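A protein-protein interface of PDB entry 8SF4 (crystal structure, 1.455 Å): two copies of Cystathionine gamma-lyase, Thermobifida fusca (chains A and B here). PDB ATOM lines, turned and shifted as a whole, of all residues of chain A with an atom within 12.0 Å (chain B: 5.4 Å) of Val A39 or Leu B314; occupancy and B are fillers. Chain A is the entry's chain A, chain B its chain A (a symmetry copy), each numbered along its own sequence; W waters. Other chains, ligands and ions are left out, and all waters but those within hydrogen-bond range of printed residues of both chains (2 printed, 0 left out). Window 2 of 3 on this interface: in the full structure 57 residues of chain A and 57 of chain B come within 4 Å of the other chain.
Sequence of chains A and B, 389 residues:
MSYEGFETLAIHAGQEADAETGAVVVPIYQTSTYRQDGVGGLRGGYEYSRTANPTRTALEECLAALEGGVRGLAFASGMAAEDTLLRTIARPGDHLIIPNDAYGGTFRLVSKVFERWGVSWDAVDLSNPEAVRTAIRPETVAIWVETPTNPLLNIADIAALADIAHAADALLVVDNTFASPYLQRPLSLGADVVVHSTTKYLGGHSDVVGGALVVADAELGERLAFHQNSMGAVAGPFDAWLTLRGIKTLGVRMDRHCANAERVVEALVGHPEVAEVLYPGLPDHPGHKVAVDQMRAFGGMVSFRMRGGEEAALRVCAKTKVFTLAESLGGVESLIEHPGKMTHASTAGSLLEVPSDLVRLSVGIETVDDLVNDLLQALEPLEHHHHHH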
ATOM      1  N   TYR A  34     -18.265 -10.737 -23.934  1.00  0.00           N
ATOM      2  CA  TYR A  34     -18.528 -11.805 -24.923  1.00  0.00           C
ATOM      3  C   TYR A  34     -19.488 -11.264 -25.967  1.00  0.00           C
ATOM      4  O   TYR A  34     -20.533 -10.704 -25.669  1.00  0.00           O
ATOM      5  CB  TYR A  34     -19.133 -13.013 -24.216  1.00  0.00           C
ATOM      6  CG  TYR A  34     -18.273 -13.500 -23.080  1.00  0.00           C
ATOM      7  CD1 TYR A  34     -18.384 -12.914 -21.819  1.00  0.00           C
ATOM      8  CD2 TYR A  34     -17.353 -14.515 -23.202  1.00  0.00           C
ATOM      9  CE1 TYR A  34     -17.582 -13.318 -20.778  1.00  0.00           C
ATOM     10  CE2 TYR A  34     -16.547 -14.938 -22.182  1.00  0.00           C
ATOM     11  CZ  TYR A  34     -16.654 -14.330 -20.935  1.00  0.00           C
ATOM     12  OH  TYR A  34     -15.778 -14.688 -19.902  1.00  0.00           O
ATOM     13  N   ARG A  35     -19.164 -11.466 -27.236  1.00  0.00           N
ATOM     14  CA  ARG A  35     -20.028 -11.150 -28.378  1.00  0.00           C
ATOM     15  C   ARG A  35     -21.278 -12.007 -28.362  1.00  0.00           C
ATOM     16  O   ARG A  35     -21.197 -13.204 -28.108  1.00  0.00           O
ATOM     17  CB  ARG A  35     -19.239 -11.406 -29.680  1.00  0.00           C
ATOM     18  CG  ARG A  35     -20.084 -11.135 -30.927  1.00  0.00           C
ATOM     19  CD  ARG A  35     -19.251 -11.356 -32.211  1.00  0.00           C
ATOM     20  NE  ARG A  35     -20.101 -11.339 -33.371  1.00  0.00           N
ATOM     21  CZ  ARG A  35     -19.677 -11.575 -34.576  1.00  0.00           C
ATOM     22  NH1 ARG A  35     -18.355 -11.724 -34.767  1.00  0.00           N
ATOM     23  NH2 ARG A  35     -20.563 -11.623 -35.554  1.00  0.00           N
ATOM     24  N   GLN A  36     -22.408 -11.382 -28.549  1.00  0.00           N
ATOM     25  CA  GLN A  36     -23.721 -12.048 -28.697  1.00  0.00           C
ATOM     26  C   GLN A  36     -24.141 -12.061 -30.147  1.00  0.00           C
ATOM     27  O   GLN A  36     -23.926 -11.062 -30.861  1.00  0.00           O
ATOM     28  CB  GLN A  36     -24.762 -11.305 -27.861  1.00  0.00           C
ATOM     29  CG  GLN A  36     -24.358 -11.252 -26.386  1.00  0.00           C
ATOM     30  CD  GLN A  36     -25.411 -10.704 -25.471  1.00  0.00           C
ATOM     31  OE1 GLN A  36     -26.597 -10.730 -25.750  1.00  0.00           O
ATOM     32  NE2 GLN A  36     -24.930 -10.279 -24.254  1.00  0.00           N
ATOM     33  N   ASP A  37     -24.808 -13.094 -30.571  1.00  0.00           N
ATOM     34  CA  ASP A  37     -25.331 -13.193 -31.952  1.00  0.00           C
ATOM     35  C   ASP A  37     -26.779 -12.691 -31.953  1.00  0.00           C
ATOM     36  O   ASP A  37     -27.740 -13.473 -31.751  1.00  0.00           O
ATOM     37  CB  ASP A  37     -25.213 -14.624 -32.445  1.00  0.00           C
ATOM     38  CG  ASP A  37     -23.758 -15.071 -32.475  1.00  0.00           C
ATOM     39  OD1 ASP A  37     -22.984 -14.388 -33.217  1.00  0.00           O
ATOM     40  OD2 ASP A  37     -23.488 -16.132 -31.897  1.00  0.00           O
ATOM     41  N   GLY A  38     -26.974 -11.392 -32.165  1.00  0.00           N
ATOM     42  CA  GLY A  38     -28.241 -10.744 -31.892  1.00  0.00           C
ATOM     43  C   GLY A  38     -28.414 -10.542 -30.388  1.00  0.00           C
ATOM     44  O   GLY A  38     -27.750 -11.158 -29.563  1.00  0.00           O
ATOM     45  N   VAL A  39     -29.319  -9.627 -30.055  1.00  0.00           N
ATOM     46  CA  VAL A  39     -29.557  -9.275 -28.637  1.00  0.00           C
ATOM     47  C   VAL A  39     -30.063 -10.498 -27.860  1.00  0.00           C
ATOM     48  O   VAL A  39     -31.069 -11.045 -28.232  1.00  0.00           O
ATOM     49  CB  VAL A  39     -30.534  -8.111 -28.537  1.00  0.00           C
ATOM     50  CG1 VAL A  39     -30.897  -7.890 -27.075  1.00  0.00           C
ATOM     51  CG2 VAL A  39     -29.871  -6.856 -29.113  1.00  0.00           C
ATOM     52  N   GLY A  40     -29.293 -10.903 -26.842  1.00  0.00           N
ATOM     53  CA  GLY A  40     -29.570 -12.129 -26.063  1.00  0.00           C
ATOM     54  C   GLY A  40     -29.135 -13.401 -26.706  1.00  0.00           C
ATOM     55  O   GLY A  40     -29.341 -14.515 -26.110  1.00  0.00           O
ATOM     56  N   GLY A  41     -28.451 -13.357 -27.869  1.00  0.00           N
ATOM     57  CA  GLY A  41     -27.972 -14.568 -28.521  1.00  0.00           C
ATOM     58  C   GLY A  41     -26.647 -15.007 -27.940  1.00  0.00           C
ATOM     59  O   GLY A  41     -25.606 -14.939 -28.623  1.00  0.00           O
ATOM     60  N   LEU A  42     -26.664 -15.595 -26.731  1.00  0.00           N
ATOM     61  CA  LEU A  42     -25.385 -15.918 -26.075  1.00  0.00           C
ATOM     62  C   LEU A  42     -24.678 -17.056 -26.780  1.00  0.00           C
ATOM     63  O   LEU A  42     -25.305 -17.966 -27.335  1.00  0.00           O
ATOM     64  CB  LEU A  42     -25.600 -16.286 -24.614  1.00  0.00           C
ATOM     65  CG  LEU A  42     -26.384 -15.296 -23.778  1.00  0.00           C
ATOM     66  CD1 LEU A  42     -26.289 -15.701 -22.315  1.00  0.00           C
ATOM     67  CD2 LEU A  42     -25.863 -13.891 -23.918  1.00  0.00           C
ATOM     68  N   ARG A  43     -23.369 -16.974 -26.775  1.00  0.00           N
ATOM     69  CA  ARG A  43     -22.497 -18.090 -27.240  1.00  0.00           C
ATOM     70  C   ARG A  43     -22.043 -18.868 -26.064  1.00  0.00           C
ATOM     71  O   ARG A  43     -21.336 -18.335 -25.089  1.00  0.00           O
ATOM     72  CB  ARG A  43     -21.259 -17.521 -27.941  1.00  0.00           C
ATOM     73  CG  ARG A  43     -21.549 -16.804 -29.176  1.00  0.00           C
ATOM     74  CD  ARG A  43     -20.328 -16.421 -29.985  1.00  0.00           C
ATOM     75  NE  ARG A  43     -20.626 -15.876 -31.264  1.00  0.00           N
ATOM     76  CZ  ARG A  43     -19.750 -15.432 -32.148  1.00  0.00           C
ATOM     77  NH1 ARG A  43     -18.421 -15.548 -31.846  1.00  0.00           N
ATOM     78  NH2 ARG A  43     -20.190 -14.860 -33.231  1.00  0.00           N
ATOM     79  N   GLY A  45     -23.486 -19.672 -23.546  1.00  0.00           N
ATOM     80  CA  GLY A  45     -24.043 -19.203 -22.303  1.00  0.00           C
ATOM     81  C   GLY A  45     -23.244 -18.086 -21.618  1.00  0.00           C
ATOM     82  O   GLY A  45     -23.622 -17.708 -20.497  1.00  0.00           O
ATOM     83  N   TYR A  46     -22.275 -17.478 -22.310  1.00  0.00           N
ATOM     84  CA  TYR A  46     -21.453 -16.452 -21.653  1.00  0.00           C
ATOM     85  C   TYR A  46     -21.914 -15.049 -22.091  1.00  0.00           C
ATOM     86  O   TYR A  46     -22.346 -14.821 -23.212  1.00  0.00           O
ATOM     87  CB  TYR A  46     -19.962 -16.687 -22.018  1.00  0.00           C
ATOM     88  CG  TYR A  46     -19.459 -17.884 -21.275  1.00  0.00           C
ATOM     89  CD1 TYR A  46     -19.095 -17.791 -19.934  1.00  0.00           C
ATOM     90  CD2 TYR A  46     -19.351 -19.149 -21.848  1.00  0.00           C
ATOM     91  CE1 TYR A  46     -18.720 -18.859 -19.165  1.00  0.00           C
ATOM     92  CE2 TYR A  46     -18.932 -20.234 -21.089  1.00  0.00           C
ATOM     93  CZ  TYR A  46     -18.640 -20.097 -19.775  1.00  0.00           C
ATOM     94  OH  TYR A  46     -18.288 -21.174 -18.966  1.00  0.00           O
ATOM     95  N   GLU A  47     -21.796 -14.149 -21.133  1.00  0.00           N
ATOM     96  CA  GLU A  47     -22.276 -12.750 -21.338  1.00  0.00           C
ATOM     97  C   GLU A  47     -21.351 -11.720 -20.657  1.00  0.00           C
ATOM     98  O   GLU A  47     -21.154 -10.630 -21.234  1.00  0.00           O
ATOM     99  CB  GLU A  47     -23.745 -12.597 -20.858  1.00  0.00           C
ATOM    100  CG  GLU A  47     -24.068 -12.743 -19.442  1.00  0.00           C
ATOM    101  CD  GLU A  47     -25.607 -12.662 -19.168  1.00  0.00           C
ATOM    102  OE1 GLU A  47     -26.324 -12.186 -20.022  1.00  0.00           O
ATOM    103  OE2 GLU A  47     -25.938 -13.398 -18.307  1.00  0.00           O
ATOM    104  N   GLY B 309     -38.575   2.596 -32.814  1.00  0.00           N
ATOM    105  CA  GLY B 309     -38.881   1.928 -31.543  1.00  0.00           C
ATOM    106  C   GLY B 309     -37.927   0.768 -31.238  1.00  0.00           C
ATOM    107  O   GLY B 309     -36.819   0.684 -31.842  1.00  0.00           O
ATOM    108  N   GLU B 310     -38.323  -0.088 -30.313  1.00  0.00           N
ATOM    109  CA  GLU B 310     -37.506  -1.250 -29.886  1.00  0.00           C
ATOM    110  C   GLU B 310     -37.139  -2.081 -31.124  1.00  0.00           C
ATOM    111  O   GLU B 310     -36.010  -2.587 -31.212  1.00  0.00           O
ATOM    112  CB  GLU B 310     -38.280  -2.091 -28.871  1.00  0.00           C
ATOM    113  CG  GLU B 310     -37.477  -3.253 -28.301  1.00  0.00           C
ATOM    114  CD  GLU B 310     -38.303  -4.105 -27.340  1.00  0.00           C
ATOM    115  OE1 GLU B 310     -39.046  -4.947 -27.804  1.00  0.00           O
ATOM    116  OE2 GLU B 310     -38.237  -3.849 -26.125  1.00  0.00           O
ATOM    117  N   GLU B 311     -38.073  -2.281 -32.031  1.00  0.00           N
ATOM    118  CA  GLU B 311     -37.823  -3.218 -33.147  1.00  0.00           C
ATOM    119  C   GLU B 311     -36.613  -2.664 -33.919  1.00  0.00           C
ATOM    120  O   GLU B 311     -35.711  -3.434 -34.266  1.00  0.00           O
ATOM    121  CB  GLU B 311     -39.132  -3.311 -33.930  1.00  0.00           C
ATOM    122  CG  GLU B 311     -39.095  -4.055 -35.229  1.00  0.00           C
ATOM    123  CD  GLU B 311     -40.459  -4.043 -35.939  1.00  0.00           C
ATOM    124  OE1 GLU B 311     -40.920  -2.976 -36.321  1.00  0.00           O
ATOM    125  OE2 GLU B 311     -41.093  -5.096 -36.040  1.00  0.00           O
ATOM    126  N   ALA B 312     -36.592  -1.359 -34.181  1.00  0.00           N
ATOM    127  CA  ALA B 312     -35.486  -0.722 -34.945  1.00  0.00           C
ATOM    128  C   ALA B 312     -34.205  -0.764 -34.140  1.00  0.00           C
ATOM    129  O   ALA B 312     -33.119  -0.980 -34.723  1.00  0.00           O
ATOM    130  CB  ALA B 312     -35.850   0.695 -35.329  1.00  0.00           C
ATOM    131  N   ALA B 313     -34.284  -0.545 -32.840  1.00  0.00           N
ATOM    132  CA  ALA B 313     -33.084  -0.572 -31.992  1.00  0.00           C
ATOM    133  C   ALA B 313     -32.458  -1.956 -31.978  1.00  0.00           C
ATOM    134  O   ALA B 313     -31.207  -2.060 -32.107  1.00  0.00           O
ATOM    135  CB  ALA B 313     -33.407  -0.091 -30.571  1.00  0.00           C
ATOM    136  N   LEU B 314     -33.243  -3.006 -31.859  1.00  0.00           N
ATOM    137  CA  LEU B 314     -32.726  -4.380 -31.869  1.00  0.00           C
ATOM    138  C   LEU B 314     -32.064  -4.679 -33.212  1.00  0.00           C
ATOM    139  O   LEU B 314     -31.007  -5.365 -33.202  1.00  0.00           O
ATOM    140  CB  LEU B 314     -33.797  -5.395 -31.507  1.00  0.00           C
ATOM    141  CG  LEU B 314     -34.449  -5.219 -30.130  1.00  0.00           C
ATOM    142  CD1 LEU B 314     -35.610  -6.179 -29.988  1.00  0.00           C
ATOM    143  CD2 LEU B 314     -33.458  -5.442 -29.026  1.00  0.00           C
ATOM    144  N   ARG B 315     -32.613  -4.170 -34.293  1.00  0.00           N
ATOM    145  CA  ARG B 315     -32.028  -4.426 -35.659  1.00  0.00           C
ATOM    146  C   ARG B 315     -30.649  -3.767 -35.765  1.00  0.00           C
ATOM    147  O   ARG B 315     -29.718  -4.432 -36.265  1.00  0.00           O
ATOM    148  CB  ARG B 315     -32.925  -3.859 -36.768  1.00  0.00           C
ATOM    149  CG  ARG B 315     -34.087  -4.764 -37.103  1.00  0.00           C
ATOM    150  CD  ARG B 315     -34.844  -4.098 -38.247  1.00  0.00           C
ATOM    151  NE  ARG B 315     -36.157  -4.669 -38.365  1.00  0.00           N
ATOM    152  CZ  ARG B 315     -37.274  -3.953 -38.250  1.00  0.00           C
ATOM    153  NH1 ARG B 315     -37.205  -2.673 -37.881  1.00  0.00           N
ATOM    154  NH2 ARG B 315     -38.439  -4.544 -38.442  1.00  0.00           N
ATOM    155  N   VAL B 316     -30.510  -2.525 -35.306  1.00  0.00           N
ATOM    156  CA  VAL B 316     -29.228  -1.791 -35.398  1.00  0.00           C
ATOM    157  C   VAL B 316     -28.191  -2.615 -34.612  1.00  0.00           C
ATOM    158  O   VAL B 316     -27.050  -2.823 -35.082  1.00  0.00           O
ATOM    159  CB  VAL B 316     -29.340  -0.356 -34.856  1.00  0.00           C
ATOM    160  CG1 VAL B 316     -27.969   0.304 -34.822  1.00  0.00           C
ATOM    161  CG2 VAL B 316     -30.324   0.502 -35.643  1.00  0.00           C
ATOM    162  N   CYS B 317     -28.555  -3.045 -33.404  1.00  0.00           N
ATOM    163  CA  CYS B 317     -27.605  -3.729 -32.529  1.00  0.00           C
ATOM    164  C   CYS B 317     -27.095  -5.019 -33.197  1.00  0.00           C
ATOM    165  O   CYS B 317     -25.933  -5.345 -32.929  1.00  0.00           O
ATOM    166  CB  CYS B 317     -28.288  -4.091 -31.213  1.00  0.00           C
ATOM    167  SG  CYS B 317     -28.515  -2.692 -30.097  1.00  0.00           S
ATOM    168  N   ALA B 318     -27.871  -5.721 -34.004  1.00  0.00           N
ATOM    169  CA  ALA B 318     -27.460  -6.980 -34.636  1.00  0.00           C
ATOM    170  C   ALA B 318     -26.680  -6.753 -35.926  1.00  0.00           C
ATOM    171  O   ALA B 318     -26.100  -7.742 -36.386  1.00  0.00           O
ATOM    172  CB  ALA B 318     -28.642  -7.854 -34.895  1.00  0.00           C
ATOM    173  N   LEU B 325     -21.525  -6.449 -30.593  1.00  0.00           N
ATOM    174  CA  LEU B 325     -22.691  -6.533 -29.683  1.00  0.00           C
ATOM    175  C   LEU B 325     -22.264  -7.324 -28.452  1.00  0.00           C
ATOM    176  O   LEU B 325     -22.037  -8.545 -28.534  1.00  0.00           O
ATOM    177  CB  LEU B 325     -23.822  -7.253 -30.406  1.00  0.00           C
ATOM    178  CG  LEU B 325     -25.121  -7.444 -29.616  1.00  0.00           C
ATOM    179  CD1 LEU B 325     -25.652  -6.096 -29.187  1.00  0.00           C
ATOM    180  CD2 LEU B 325     -26.135  -8.110 -30.495  1.00  0.00           C
ATOM    181  N   HIS B 338     -28.164  -3.047 -26.358  1.00  0.00           N
ATOM    182  CA  HIS B 338     -29.532  -2.610 -26.087  1.00  0.00           C
ATOM    183  C   HIS B 338     -29.746  -2.677 -24.585  1.00  0.00           C
ATOM    184  O   HIS B 338     -29.954  -3.756 -24.066  1.00  0.00           O
ATOM    185  CB  HIS B 338     -30.520  -3.538 -26.801  1.00  0.00           C
ATOM    186  CG  HIS B 338     -31.929  -3.093 -26.625  1.00  0.00           C
ATOM    187  ND1 HIS B 338     -32.764  -3.636 -25.663  1.00  0.00           N
ATOM    188  CD2 HIS B 338     -32.630  -2.183 -27.337  1.00  0.00           C
ATOM    189  CE1 HIS B 338     -33.939  -3.008 -25.820  1.00  0.00           C
ATOM    190  NE2 HIS B 338     -33.881  -2.106 -26.771  1.00  0.00           N
ATOM    191  N   LYS B 341     -32.839  -4.842 -22.904  1.00  0.00           N
ATOM    192  CA  LYS B 341     -32.797  -6.327 -22.863  1.00  0.00           C
ATOM    193  C   LYS B 341     -31.463  -6.871 -22.383  1.00  0.00           C
ATOM    194  O   LYS B 341     -31.434  -8.075 -22.059  1.00  0.00           O
ATOM    195  CB  LYS B 341     -33.110  -6.904 -24.243  1.00  0.00           C
ATOM    196  CG  LYS B 341     -34.543  -6.650 -24.658  1.00  0.00           C
ATOM    197  CD  LYS B 341     -34.914  -7.316 -25.908  1.00  0.00           C
ATOM    198  CE  LYS B 341     -36.390  -7.208 -26.295  1.00  0.00           C
ATOM    199  NZ  LYS B 341     -37.387  -7.202 -25.185  1.00  0.00           N
ATOM    200  N   MET B 342     -30.407  -6.031 -22.285  1.00  0.00           N
ATOM    201  CA  MET B 342     -29.077  -6.522 -21.905  1.00  0.00           C
ATOM    202  C   MET B 342     -28.730  -5.952 -20.543  1.00  0.00           C
ATOM    203  O   MET B 342     -29.231  -6.462 -19.520  1.00  0.00           O
ATOM    204  CB  MET B 342     -28.106  -6.241 -23.064  1.00  0.00           C
ATOM    205  CG  MET B 342     -28.456  -7.011 -24.322  1.00  0.00           C
ATOM    206  SD  MET B 342     -27.480  -6.480 -25.780  1.00  0.00           S
ATOM    207  CE  MET B 342     -25.787  -6.945 -25.264  1.00  0.00           C
HETATM  208  O   HOH W   1     -25.259  -9.763 -34.181  1.00  0.00           O
HETATM  209  O   HOH W   2     -30.791  -8.092 -32.079  1.00  0.00           O
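No position is printed for both chains. Of the 10 pairs that touch across the chains among the printed residues, none has its exchanged pair printed and touching as well.
Of the 14 printed residues of chain B, 5 touch a printed residue of chain A. Of the 13 printed residues of chain A, 5 touch a printed residue of chain B. Printed residues of chain A that touch a printed residue of chain B: Tyr A34, Arg A35, Gln A36, Gly A38 and Val A39. Hydrophobic or aromatic side chains of chain A within 4 Å of the printed part of chain B: Val A39. Among the printed residues, no Asp or Glu carboxylate lies within 4 Å of a Lys or Arg side-chain nitrogen of the other chain.
The backbone NH (N) of Gln A36 lies within hydrogen-bond range of the backbone carbonyl oxygen (O) of Leu B325.
Water W2 bridges N of Val A39 and O of Leu B314. Water W1 bridges the backbone carbonyl oxygen (O) of Ala B318 (3.1 Å) and the backbone NH (N) of Gly A38 (3.1 Å).
Tyr A34 touches Leu B325. CA of Arg A35 touches O of Leu B325, 3.3 Å away. CE of Met B342 touches NE2 of Gln A36, at 3.6 Å. Gly A38 touches Leu B325. Leu B314 touches Val A39 (CD2 to CG2, 3.9 Å). Cys B317 touches Val A39 (CB to CG2, 3.8 Å). CD2 of Leu B325 touches N of Val A39 (3.6 Å). Val A39 touches Lys B341 (CG1 to CB, 3.7 Å). Met B342 touches Val A39 (CG to CG1, 3.8 Å).
Of chain B, only Leu B314 (3.9 Å), Cys B317 (3.8 Å), Leu B325 (3.6 Å), Lys B341 (3.7 Å) and Met B342 (3.8 Å) come within 4 Å of Val A39. Of chain A, only Val A39 (3.9 Å) comes within 4 Å of Leu B314. No residue of chain A comes within 4 Å of Gly B309. No residue of chain A comes within 4 Å of Ala B313. Of the printed residues of chain A, Cys B317 touches Val A39. His B338 touches none of the printed residues of chain A. Lys B341 touches one residue of chain A. Met B342 touches just these residues of chain A: Gln A36 (3.6 Å) and Val A39 (3.8 Å). Of the printed residues of chain A, Leu B325 touches Tyr A34 (3.9 Å), Arg A35 (3.3 Å), Gln A36 (2.9 Å), Gly A38 (3.3 Å) and Val A39 (3.6 Å). Of the printed residues of chain B, Gly A38 touches Leu B325. Printed residues of chain B within 4 Å of Tyr A34: Leu B325. Of the printed residues of chain B, Gln A36 touches Leu B325 (2.9 Å) and Met B342 (3.6 Å). Of the printed residues of chain B, Arg A35 touches Leu B325. Arg B315 touches none of the printed residues of chain A. The nearest residue of chain B that does not touch Val A39 is His B338 (4.1 Å). The nearest residue of chain A that does not touch Leu B314 is Gly A38 (6.2 Å).
The backbone NH (N) of Gly A40 is in hydrogen-bond range of the side-chain amide oxygen (OE1) of Gln A36. The side-chain carboxylate (OE2) of Glu B310 lies within salt-bridge range of the side-chain amino group (NZ) of Lys B341 (3.6 Å). SG of Cys B317 sits at hydrogen-bond distance from O of Ala B313, 3.4 Å away. The side-chain sulfur of Cys B317 lies within hydrogen-bond range of the backbone NH of His B338 (3.8 Å). A ring nitrogen (ND1) of His B338 lies within hydrogen-bond range of the backbone NH of Lys B341, 3.0 Å away. N of His B338 sits at hydrogen-bond distance from SD of Met B342, 3.5 Å away.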
